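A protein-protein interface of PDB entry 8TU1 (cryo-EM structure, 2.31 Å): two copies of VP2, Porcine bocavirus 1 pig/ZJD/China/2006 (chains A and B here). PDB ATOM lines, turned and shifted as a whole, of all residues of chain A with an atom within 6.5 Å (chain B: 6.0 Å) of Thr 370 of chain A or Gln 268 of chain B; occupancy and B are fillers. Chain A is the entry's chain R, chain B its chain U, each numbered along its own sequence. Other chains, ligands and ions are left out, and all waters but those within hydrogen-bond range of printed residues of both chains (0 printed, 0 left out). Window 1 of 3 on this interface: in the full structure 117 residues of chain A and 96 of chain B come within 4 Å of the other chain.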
ATOM      1  N   GLY A 328      -6.727 -24.252 -27.673  1.00  0.00           N
ATOM      2  CA  GLY A 328      -6.509 -23.301 -28.732  1.00  0.00           C
ATOM      3  C   GLY A 328      -6.353 -21.884 -28.244  1.00  0.00           C
ATOM      4  O   GLY A 328      -5.996 -21.658 -27.098  1.00  0.00           O
ATOM      5  N   PRO A 329      -6.622 -20.915 -29.126  1.00  0.00           N
ATOM      6  CA  PRO A 329      -6.874 -21.134 -30.552  1.00  0.00           C
ATOM      7  C   PRO A 329      -5.629 -21.542 -31.326  1.00  0.00           C
ATOM      8  O   PRO A 329      -5.730 -22.148 -32.383  1.00  0.00           O
ATOM      9  CB  PRO A 329      -7.384 -19.775 -31.017  1.00  0.00           C
ATOM     10  CG  PRO A 329      -7.976 -19.187 -29.818  1.00  0.00           C
ATOM     11  CD  PRO A 329      -7.074 -19.585 -28.709  1.00  0.00           C
ATOM     12  N   ILE A 330      -4.465 -21.197 -30.795  1.00  0.00           N
ATOM     13  CA  ILE A 330      -3.186 -21.609 -31.350  1.00  0.00           C
ATOM     14  C   ILE A 330      -2.588 -22.645 -30.418  1.00  0.00           C
ATOM     15  O   ILE A 330      -2.395 -22.379 -29.227  1.00  0.00           O
ATOM     16  CB  ILE A 330      -2.229 -20.421 -31.539  1.00  0.00           C
ATOM     17  CG1 ILE A 330      -2.822 -19.415 -32.519  1.00  0.00           C
ATOM     18  CG2 ILE A 330      -0.873 -20.892 -32.014  1.00  0.00           C
ATOM     19  CD1 ILE A 330      -3.057 -19.995 -33.876  1.00  0.00           C
ATOM     20  N   VAL A 331      -2.302 -23.823 -30.954  1.00  0.00           N
ATOM     21  CA  VAL A 331      -1.624 -24.879 -30.216  1.00  0.00           C
ATOM     22  C   VAL A 331      -0.259 -25.090 -30.850  1.00  0.00           C
ATOM     23  O   VAL A 331      -0.157 -25.295 -32.063  1.00  0.00           O
ATOM     24  CB  VAL A 331      -2.432 -26.186 -30.209  1.00  0.00           C
ATOM     25  CG1 VAL A 331      -1.649 -27.272 -29.500  1.00  0.00           C
ATOM     26  CG2 VAL A 331      -3.771 -25.970 -29.546  1.00  0.00           C
ATOM     27  N   THR A 332       0.781 -25.034 -30.033  1.00  0.00           N
ATOM     28  CA  THR A 332       2.150 -25.200 -30.491  1.00  0.00           C
ATOM     29  C   THR A 332       2.706 -26.509 -29.962  1.00  0.00           C
ATOM     30  O   THR A 332       2.708 -26.743 -28.751  1.00  0.00           O
ATOM     31  CB  THR A 332       3.026 -24.034 -30.032  1.00  0.00           C
ATOM     32  OG1 THR A 332       2.531 -22.814 -30.589  1.00  0.00           O
ATOM     33  CG2 THR A 332       4.451 -24.232 -30.478  1.00  0.00           C
ATOM     34  N   ILE A 334       6.055 -28.465 -29.469  1.00  0.00           N
ATOM     35  CA  ILE A 334       7.502 -28.405 -29.431  1.00  0.00           C
ATOM     36  C   ILE A 334       8.006 -29.834 -29.466  1.00  0.00           C
ATOM     37  O   ILE A 334       7.517 -30.691 -28.722  1.00  0.00           O
ATOM     38  CB  ILE A 334       8.017 -27.671 -28.186  1.00  0.00           C
ATOM     39  CG1 ILE A 334       7.429 -26.265 -28.100  1.00  0.00           C
ATOM     40  CG2 ILE A 334       9.514 -27.542 -28.254  1.00  0.00           C
ATOM     41  CD1 ILE A 334       7.796 -25.377 -29.260  1.00  0.00           C
ATOM     42  N   TRP A 368       1.123 -26.871 -26.593  1.00  0.00           N
ATOM     43  CA  TRP A 368       1.003 -25.753 -25.676  1.00  0.00           C
ATOM     44  C   TRP A 368       0.170 -24.681 -26.356  1.00  0.00           C
ATOM     45  O   TRP A 368       0.392 -24.373 -27.531  1.00  0.00           O
ATOM     46  CB  TRP A 368       2.373 -25.215 -25.267  1.00  0.00           C
ATOM     47  CG  TRP A 368       3.194 -26.232 -24.561  1.00  0.00           C
ATOM     48  CD1 TRP A 368       4.215 -26.954 -25.082  1.00  0.00           C
ATOM     49  CD2 TRP A 368       2.985 -26.731 -23.243  1.00  0.00           C
ATOM     50  NE1 TRP A 368       4.703 -27.823 -24.153  1.00  0.00           N
ATOM     51  CE2 TRP A 368       3.957 -27.717 -23.013  1.00  0.00           C
ATOM     52  CE3 TRP A 368       2.087 -26.427 -22.227  1.00  0.00           C
ATOM     53  CZ2 TRP A 368       4.058 -28.397 -21.809  1.00  0.00           C
ATOM     54  CZ3 TRP A 368       2.188 -27.096 -21.040  1.00  0.00           C
ATOM     55  CH2 TRP A 368       3.166 -28.070 -20.836  1.00  0.00           C
ATOM     56  N   GLN A 369      -0.784 -24.123 -25.631  1.00  0.00           N
ATOM     57  CA  GLN A 369      -1.807 -23.271 -26.213  1.00  0.00           C
ATOM     58  C   GLN A 369      -1.558 -21.797 -25.932  1.00  0.00           C
ATOM     59  O   GLN A 369      -1.092 -21.421 -24.855  1.00  0.00           O
ATOM     60  CB  GLN A 369      -3.183 -23.691 -25.703  1.00  0.00           C
ATOM     61  CG  GLN A 369      -3.293 -23.684 -24.209  1.00  0.00           C
ATOM     62  CD  GLN A 369      -4.643 -24.130 -23.726  1.00  0.00           C
ATOM     63  OE1 GLN A 369      -5.436 -24.681 -24.482  1.00  0.00           O
ATOM     64  NE2 GLN A 369      -4.890 -23.955 -22.443  1.00  0.00           N
ATOM     65  N   THR A 370      -1.863 -20.971 -26.924  1.00  0.00           N
ATOM     66  CA  THR A 370      -1.790 -19.521 -26.828  1.00  0.00           C
ATOM     67  C   THR A 370      -3.204 -18.973 -26.954  1.00  0.00           C
ATOM     68  O   THR A 370      -3.848 -19.155 -27.989  1.00  0.00           O
ATOM     69  CB  THR A 370      -0.886 -18.940 -27.921  1.00  0.00           C
ATOM     70  OG1 THR A 370       0.435 -19.460 -27.779  1.00  0.00           O
ATOM     71  CG2 THR A 370      -0.823 -17.425 -27.835  1.00  0.00           C
ATOM     72  N   ALA A 371      -3.698 -18.348 -25.892  1.00  0.00           N
ATOM     73  CA  ALA A 371      -5.003 -17.700 -25.916  1.00  0.00           C
ATOM     74  C   ALA A 371      -5.002 -16.474 -25.022  1.00  0.00           C
ATOM     75  O   ALA A 371      -4.334 -16.468 -24.000  1.00  0.00           O
ATOM     76  CB  ALA A 371      -6.076 -18.667 -25.477  1.00  0.00           C
ATOM     77  N   PRO A 372      -5.756 -15.433 -25.392  1.00  0.00           N
ATOM     78  CA  PRO A 372      -6.466 -15.215 -26.655  1.00  0.00           C
ATOM     79  C   PRO A 372      -5.515 -14.810 -27.771  1.00  0.00           C
ATOM     80  O   PRO A 372      -4.485 -14.215 -27.507  1.00  0.00           O
ATOM     81  CB  PRO A 372      -7.418 -14.077 -26.320  1.00  0.00           C
ATOM     82  CG  PRO A 372      -6.708 -13.312 -25.290  1.00  0.00           C
ATOM     83  CD  PRO A 372      -5.933 -14.295 -24.478  1.00  0.00           C
ATOM     84  N   VAL A 373      -5.901 -15.016 -29.021  1.00  0.00           N
ATOM     85  CA  VAL A 373      -5.059 -14.606 -30.141  1.00  0.00           C
ATOM     86  C   VAL A 373      -5.866 -13.760 -31.112  1.00  0.00           C
ATOM     87  O   VAL A 373      -5.541 -13.664 -32.287  1.00  0.00           O
ATOM     88  CB  VAL A 373      -4.510 -15.814 -30.913  1.00  0.00           C
ATOM     89  CG1 VAL A 373      -3.600 -16.654 -30.032  1.00  0.00           C
ATOM     90  CG2 VAL A 373      -5.654 -16.639 -31.473  1.00  0.00           C
ATOM     91  N   CYS B 266       9.576 -23.852 -23.834  1.00  0.00           N
ATOM     92  CA  CYS B 266       8.920 -22.834 -24.628  1.00  0.00           C
ATOM     93  C   CYS B 266       8.253 -21.827 -23.700  1.00  0.00           C
ATOM     94  O   CYS B 266       7.972 -22.137 -22.543  1.00  0.00           O
ATOM     95  CB  CYS B 266       7.878 -23.442 -25.559  1.00  0.00           C
ATOM     96  SG  CYS B 266       6.564 -24.353 -24.762  1.00  0.00           S
ATOM     97  N   PRO B 267       8.002 -20.614 -24.181  1.00  0.00           N
ATOM     98  CA  PRO B 267       7.284 -19.640 -23.349  1.00  0.00           C
ATOM     99  C   PRO B 267       5.930 -20.128 -22.893  1.00  0.00           C
ATOM    100  O   PRO B 267       5.441 -19.691 -21.848  1.00  0.00           O
ATOM    101  CB  PRO B 267       7.157 -18.433 -24.283  1.00  0.00           C
ATOM    102  CG  PRO B 267       8.285 -18.563 -25.196  1.00  0.00           C
ATOM    103  CD  PRO B 267       8.449 -20.019 -25.444  1.00  0.00           C
ATOM    104  N   GLN B 268       5.317 -21.040 -23.634  1.00  0.00           N
ATOM    105  CA  GLN B 268       3.956 -21.460 -23.355  1.00  0.00           C
ATOM    106  C   GLN B 268       3.868 -22.536 -22.285  1.00  0.00           C
ATOM    107  O   GLN B 268       2.767 -22.815 -21.808  1.00  0.00           O
ATOM    108  CB  GLN B 268       3.309 -21.959 -24.643  1.00  0.00           C
ATOM    109  CG  GLN B 268       3.158 -20.915 -25.726  1.00  0.00           C
ATOM    110  CD  GLN B 268       4.436 -20.698 -26.513  1.00  0.00           C
ATOM    111  OE1 GLN B 268       5.466 -21.298 -26.224  1.00  0.00           O
ATOM    112  NE2 GLN B 268       4.370 -19.842 -27.520  1.00  0.00           N
ATOM    113  N   SER B 269       4.978 -23.177 -21.923  1.00  0.00           N
ATOM    114  CA  SER B 269       4.989 -24.185 -20.869  1.00  0.00           C
ATOM    115  C   SER B 269       5.439 -23.617 -19.527  1.00  0.00           C
ATOM    116  O   SER B 269       5.479 -24.341 -18.531  1.00  0.00           O
ATOM    117  CB  SER B 269       5.884 -25.357 -21.265  1.00  0.00           C
ATOM    118  OG  SER B 269       7.238 -24.960 -21.353  1.00  0.00           O
ATOM    119  N   ASP B 270       5.726 -22.327 -19.478  1.00  0.00           N
ATOM    120  CA  ASP B 270       6.677 -21.742 -18.548  1.00  0.00           C
ATOM    121  C   ASP B 270       6.030 -21.316 -17.229  1.00  0.00           C
ATOM    122  O   ASP B 270       6.637 -20.572 -16.463  1.00  0.00           O
ATOM    123  CB  ASP B 270       7.380 -20.566 -19.229  1.00  0.00           C
ATOM    124  CG  ASP B 270       8.677 -20.177 -18.556  1.00  0.00           C
ATOM    125  OD1 ASP B 270       9.105 -20.872 -17.614  1.00  0.00           O
ATOM    126  OD2 ASP B 270       9.281 -19.173 -18.988  1.00  0.00           O
ATOM    127  N   PHE B 271       4.777 -21.681 -17.003  1.00  0.00           N
ATOM    128  CA  PHE B 271       3.977 -21.317 -15.844  1.00  0.00           C
ATOM    129  C   PHE B 271       4.227 -22.227 -14.635  1.00  0.00           C
ATOM    130  O   PHE B 271       5.085 -23.109 -14.640  1.00  0.00           O
ATOM    131  CB  PHE B 271       2.508 -21.358 -16.230  1.00  0.00           C
ATOM    132  CG  PHE B 271       2.113 -22.639 -16.875  1.00  0.00           C
ATOM    133  CD1 PHE B 271       1.742 -23.729 -16.118  1.00  0.00           C
ATOM    134  CD2 PHE B 271       2.140 -22.763 -18.249  1.00  0.00           C
ATOM    135  CE1 PHE B 271       1.397 -24.903 -16.722  1.00  0.00           C
ATOM    136  CE2 PHE B 271       1.789 -23.933 -18.852  1.00  0.00           C
ATOM    137  CZ  PHE B 271       1.417 -25.004 -18.089  1.00  0.00           C
ATOM    138  N   LYS B 301      -1.689 -23.703 -19.053  1.00  0.00           N
ATOM    139  CA  LYS B 301      -2.221 -22.375 -18.904  1.00  0.00           C
ATOM    140  C   LYS B 301      -2.096 -21.644 -20.229  1.00  0.00           C
ATOM    141  O   LYS B 301      -1.033 -21.667 -20.852  1.00  0.00           O
ATOM    142  CB  LYS B 301      -1.501 -21.627 -17.792  1.00  0.00           C
ATOM    143  CG  LYS B 301      -1.806 -22.194 -16.435  1.00  0.00           C
ATOM    144  CD  LYS B 301      -1.067 -21.484 -15.343  1.00  0.00           C
ATOM    145  CE  LYS B 301      -1.448 -22.046 -14.002  1.00  0.00           C
ATOM    146  NZ  LYS B 301      -0.705 -21.399 -12.902  1.00  0.00           N
ATOM    147  N   PRO B 302      -3.168 -21.040 -20.708  1.00  0.00           N
ATOM    148  CA  PRO B 302      -3.082 -20.281 -21.953  1.00  0.00           C
ATOM    149  C   PRO B 302      -2.019 -19.205 -21.855  1.00  0.00           C
ATOM    150  O   PRO B 302      -1.870 -18.536 -20.833  1.00  0.00           O
ATOM    151  CB  PRO B 302      -4.485 -19.689 -22.099  1.00  0.00           C
ATOM    152  CG  PRO B 302      -4.995 -19.651 -20.719  1.00  0.00           C
ATOM    153  CD  PRO B 302      -4.451 -20.838 -20.029  1.00  0.00           C
ATOM    154  N   SER B 303      -1.276 -19.051 -22.932  1.00  0.00           N
ATOM    155  CA  SER B 303      -0.130 -18.166 -22.972  1.00  0.00           C
ATOM    156  C   SER B 303      -0.465 -16.944 -23.808  1.00  0.00           C
ATOM    157  O   SER B 303      -1.291 -17.004 -24.717  1.00  0.00           O
ATOM    158  CB  SER B 303       1.091 -18.878 -23.556  1.00  0.00           C
ATOM    159  OG  SER B 303       2.202 -18.011 -23.646  1.00  0.00           O
ATOM    160  N   ASN B 304       0.162 -15.829 -23.472  1.00  0.00           N
ATOM    161  CA  ASN B 304       0.081 -14.648 -24.312  1.00  0.00           C
ATOM    162  C   ASN B 304       1.053 -14.685 -25.474  1.00  0.00           C
ATOM    163  O   ASN B 304       1.051 -13.758 -26.283  1.00  0.00           O
ATOM    164  CB  ASN B 304       0.334 -13.391 -23.485  1.00  0.00           C
ATOM    165  CG  ASN B 304      -0.825 -13.050 -22.600  1.00  0.00           C
ATOM    166  OD1 ASN B 304      -1.959 -13.420 -22.888  1.00  0.00           O
ATOM    167  ND2 ASN B 304      -0.553 -12.363 -21.498  1.00  0.00           N
ATOM    168  N   TRP B 305       1.871 -15.716 -25.592  1.00  0.00           N
ATOM    169  CA  TRP B 305       2.999 -15.677 -26.503  1.00  0.00           C
ATOM    170  C   TRP B 305       2.779 -16.656 -27.645  1.00  0.00           C
ATOM    171  O   TRP B 305       2.552 -17.846 -27.422  1.00  0.00           O
ATOM    172  CB  TRP B 305       4.298 -15.948 -25.755  1.00  0.00           C
ATOM    173  CG  TRP B 305       4.498 -14.889 -24.748  1.00  0.00           C
ATOM    174  CD1 TRP B 305       4.321 -14.992 -23.407  1.00  0.00           C
ATOM    175  CD2 TRP B 305       4.733 -13.509 -25.014  1.00  0.00           C
ATOM    176  NE1 TRP B 305       4.524 -13.782 -22.810  1.00  0.00           N
ATOM    177  CE2 TRP B 305       4.766 -12.849 -23.778  1.00  0.00           C
ATOM    178  CE3 TRP B 305       4.956 -12.777 -26.174  1.00  0.00           C
ATOM    179  CZ2 TRP B 305       5.020 -11.492 -23.670  1.00  0.00           C
ATOM    180  CZ3 TRP B 305       5.205 -11.440 -26.067  1.00  0.00           C
ATOM    181  CH2 TRP B 305       5.238 -10.807 -24.828  1.00  0.00           C
ATOM    182  N   MET B 306       2.823 -16.140 -28.841  1.00  0.00           N
ATOM    183  CA  MET B 306       2.655 -16.844 -30.093  1.00  0.00           C
ATOM    184  C   MET B 306       3.929 -17.574 -30.487  1.00  0.00           C
ATOM    185  O   MET B 306       5.033 -17.088 -30.240  1.00  0.00           O
ATOM    186  CB  MET B 306       2.287 -15.862 -31.193  1.00  0.00           C
ATOM    187  CG  MET B 306       0.910 -15.284 -31.076  1.00  0.00           C
ATOM    188  SD  MET B 306      -0.330 -16.555 -31.295  1.00  0.00           S
ATOM    189  CE  MET B 306      -0.068 -16.934 -33.018  1.00  0.00           C
ATOM    190  N   PRO B 307       3.798 -18.738 -31.103  1.00  0.00           N
ATOM    191  CA  PRO B 307       4.949 -19.342 -31.769  1.00  0.00           C
ATOM    192  C   PRO B 307       5.467 -18.409 -32.846  1.00  0.00           C
ATOM    193  O   PRO B 307       4.704 -17.762 -33.565  1.00  0.00           O
ATOM    194  CB  PRO B 307       4.376 -20.627 -32.366  1.00  0.00           C
ATOM    195  CG  PRO B 307       2.947 -20.314 -32.563  1.00  0.00           C
ATOM    196  CD  PRO B 307       2.555 -19.459 -31.402  1.00  0.00           C
ATOM    197  N   MET B 407      14.014 -24.845 -27.384  1.00  0.00           N
ATOM    198  CA  MET B 407      12.629 -25.242 -27.157  1.00  0.00           C
ATOM    199  C   MET B 407      11.649 -24.124 -27.495  1.00  0.00           C
ATOM    200  O   MET B 407      10.436 -24.303 -27.374  1.00  0.00           O
ATOM    201  CB  MET B 407      12.459 -25.708 -25.714  1.00  0.00           C
ATOM    202  CG  MET B 407      13.329 -26.910 -25.385  1.00  0.00           C
ATOM    203  SD  MET B 407      13.041 -28.396 -26.358  1.00  0.00           S
ATOM    204  CE  MET B 407      11.458 -28.914 -25.728  1.00  0.00           C
ATOM    205  N   VAL B 438       7.521 -14.722 -30.305  1.00  0.00           N
ATOM    206  CA  VAL B 438       8.774 -14.695 -29.575  1.00  0.00           C
ATOM    207  C   VAL B 438       9.499 -15.987 -29.923  1.00  0.00           C
ATOM    208  O   VAL B 438       8.901 -17.063 -29.872  1.00  0.00           O
ATOM    209  CB  VAL B 438       8.494 -14.533 -28.062  1.00  0.00           C
ATOM    210  CG1 VAL B 438       7.828 -15.761 -27.441  1.00  0.00           C
ATOM    211  CG2 VAL B 438       9.670 -14.087 -27.309  1.00  0.00           C
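The backbone NH (N) of Ala 371 of chain A lies within hydrogen-bond range of the backbone carbonyl oxygen (O) of Ser 303 of chain B. The backbone NH (N) of Ser 303 of chain B lies within hydrogen-bond range of the backbone carbonyl oxygen (O) of Gln 369 of chain A. The side-chain hydroxyl (OG1) of Thr 370 of chain A sits at hydrogen-bond distance from the backbone carbonyl oxygen (O) of Trp 305 of chain B, 2.7 Å away.
O of Trp 305 of chain B lies within hydrogen-bond range of NE2 of Gln 268 of chain B, 2.7 Å away. The side-chain hydroxyl (OG) of Ser 303 of chain B lies within hydrogen-bond range of the backbone NH (N) of Trp 305 of chain B, at 3.0 Å. O of Cys 266 of chain B lies within hydrogen-bond range of OG of Ser 269 of chain B (3.2 Å). The side-chain sulfur (SG) of Cys 266 of chain B lies close to the side-chain amide oxygen (OE1) of Gln 268 of chain B, 3.6 Å away. N of Thr 332 of chain A is in hydrogen-bond range of O of Trp 368 of chain A. O of Met 306 of chain B is in hydrogen-bond range of N of Val 438 of chain B, 3.4 Å away.
Ile 330 of chain A touches Met 306 of chain B (CG1 to CE, 3.7 Å). Ile 330 of chain A touches Pro 307 of chain B (CG2 to CD, 3.8 Å). Thr 332 of chain A touches Pro 307 of chain B. Cys 266 of chain B touches Ile 334 of chain A (CB to CG1, 3.8 Å). Trp 368 of chain A touches Cys 266 of chain B (CD1 to SG, 3.5 Å). CB of Gln 268 of chain B touches CB of Trp 368 of chain A (3.4 Å). Phe 271 of chain B touches Trp 368 of chain A (CZ to CZ3, 3.7 Å). Gln 369 of chain A touches Pro 302 of chain B (O to CA, 3.7 Å). Thr 370 of chain A touches Ser 303 of chain B. SD of Met 306 of chain B touches CG2 of Thr 370 of chain A (3.6 Å).
Printed residues of chain B within 4 Å of Ile 330 of chain A: Met 306 (3.7 Å) and Pro 307 (3.8 Å). Printed residues of chain B within 4 Å of Gln 369 of chain A: Pro 302 and Ser 303. Of chain B, only Gln 268, Ser 303, Trp 305 and Met 306 come within 4 Å of Thr 370 of chain A. Printed residues of chain A within 4 Å of Gln 268 of chain B: Trp 368 (3.4 Å) and Thr 370 (3.7 Å). Of the printed residues of chain A, Phe 271 of chain B touches Trp 368. Printed residues of chain A within 4 Å of Pro 302 of chain B: Gln 369 (3.7 Å) and Ala 371 (3.7 Å). The nearest residue of chain B that does not touch Thr 370 of chain A is Asn 304 of chain B (4.1 Å). The nearest residue of chain A that does not touch Gln 268 of chain B is Gln 369 of chain A (4.4 Å). The nearest printed residue of chain B that does not touch Gln 369 of chain A is Lys 301 of chain B (4.01 Å).
Hydrophobic or aromatic side chains of chain A within 4 Å of the printed part of chain B: Ile 330, Ile 334, Trp 368, Ala 371 and Val 373. Among the printed residues, 18 pairs touch across the chains.
No position is printed for both chains.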
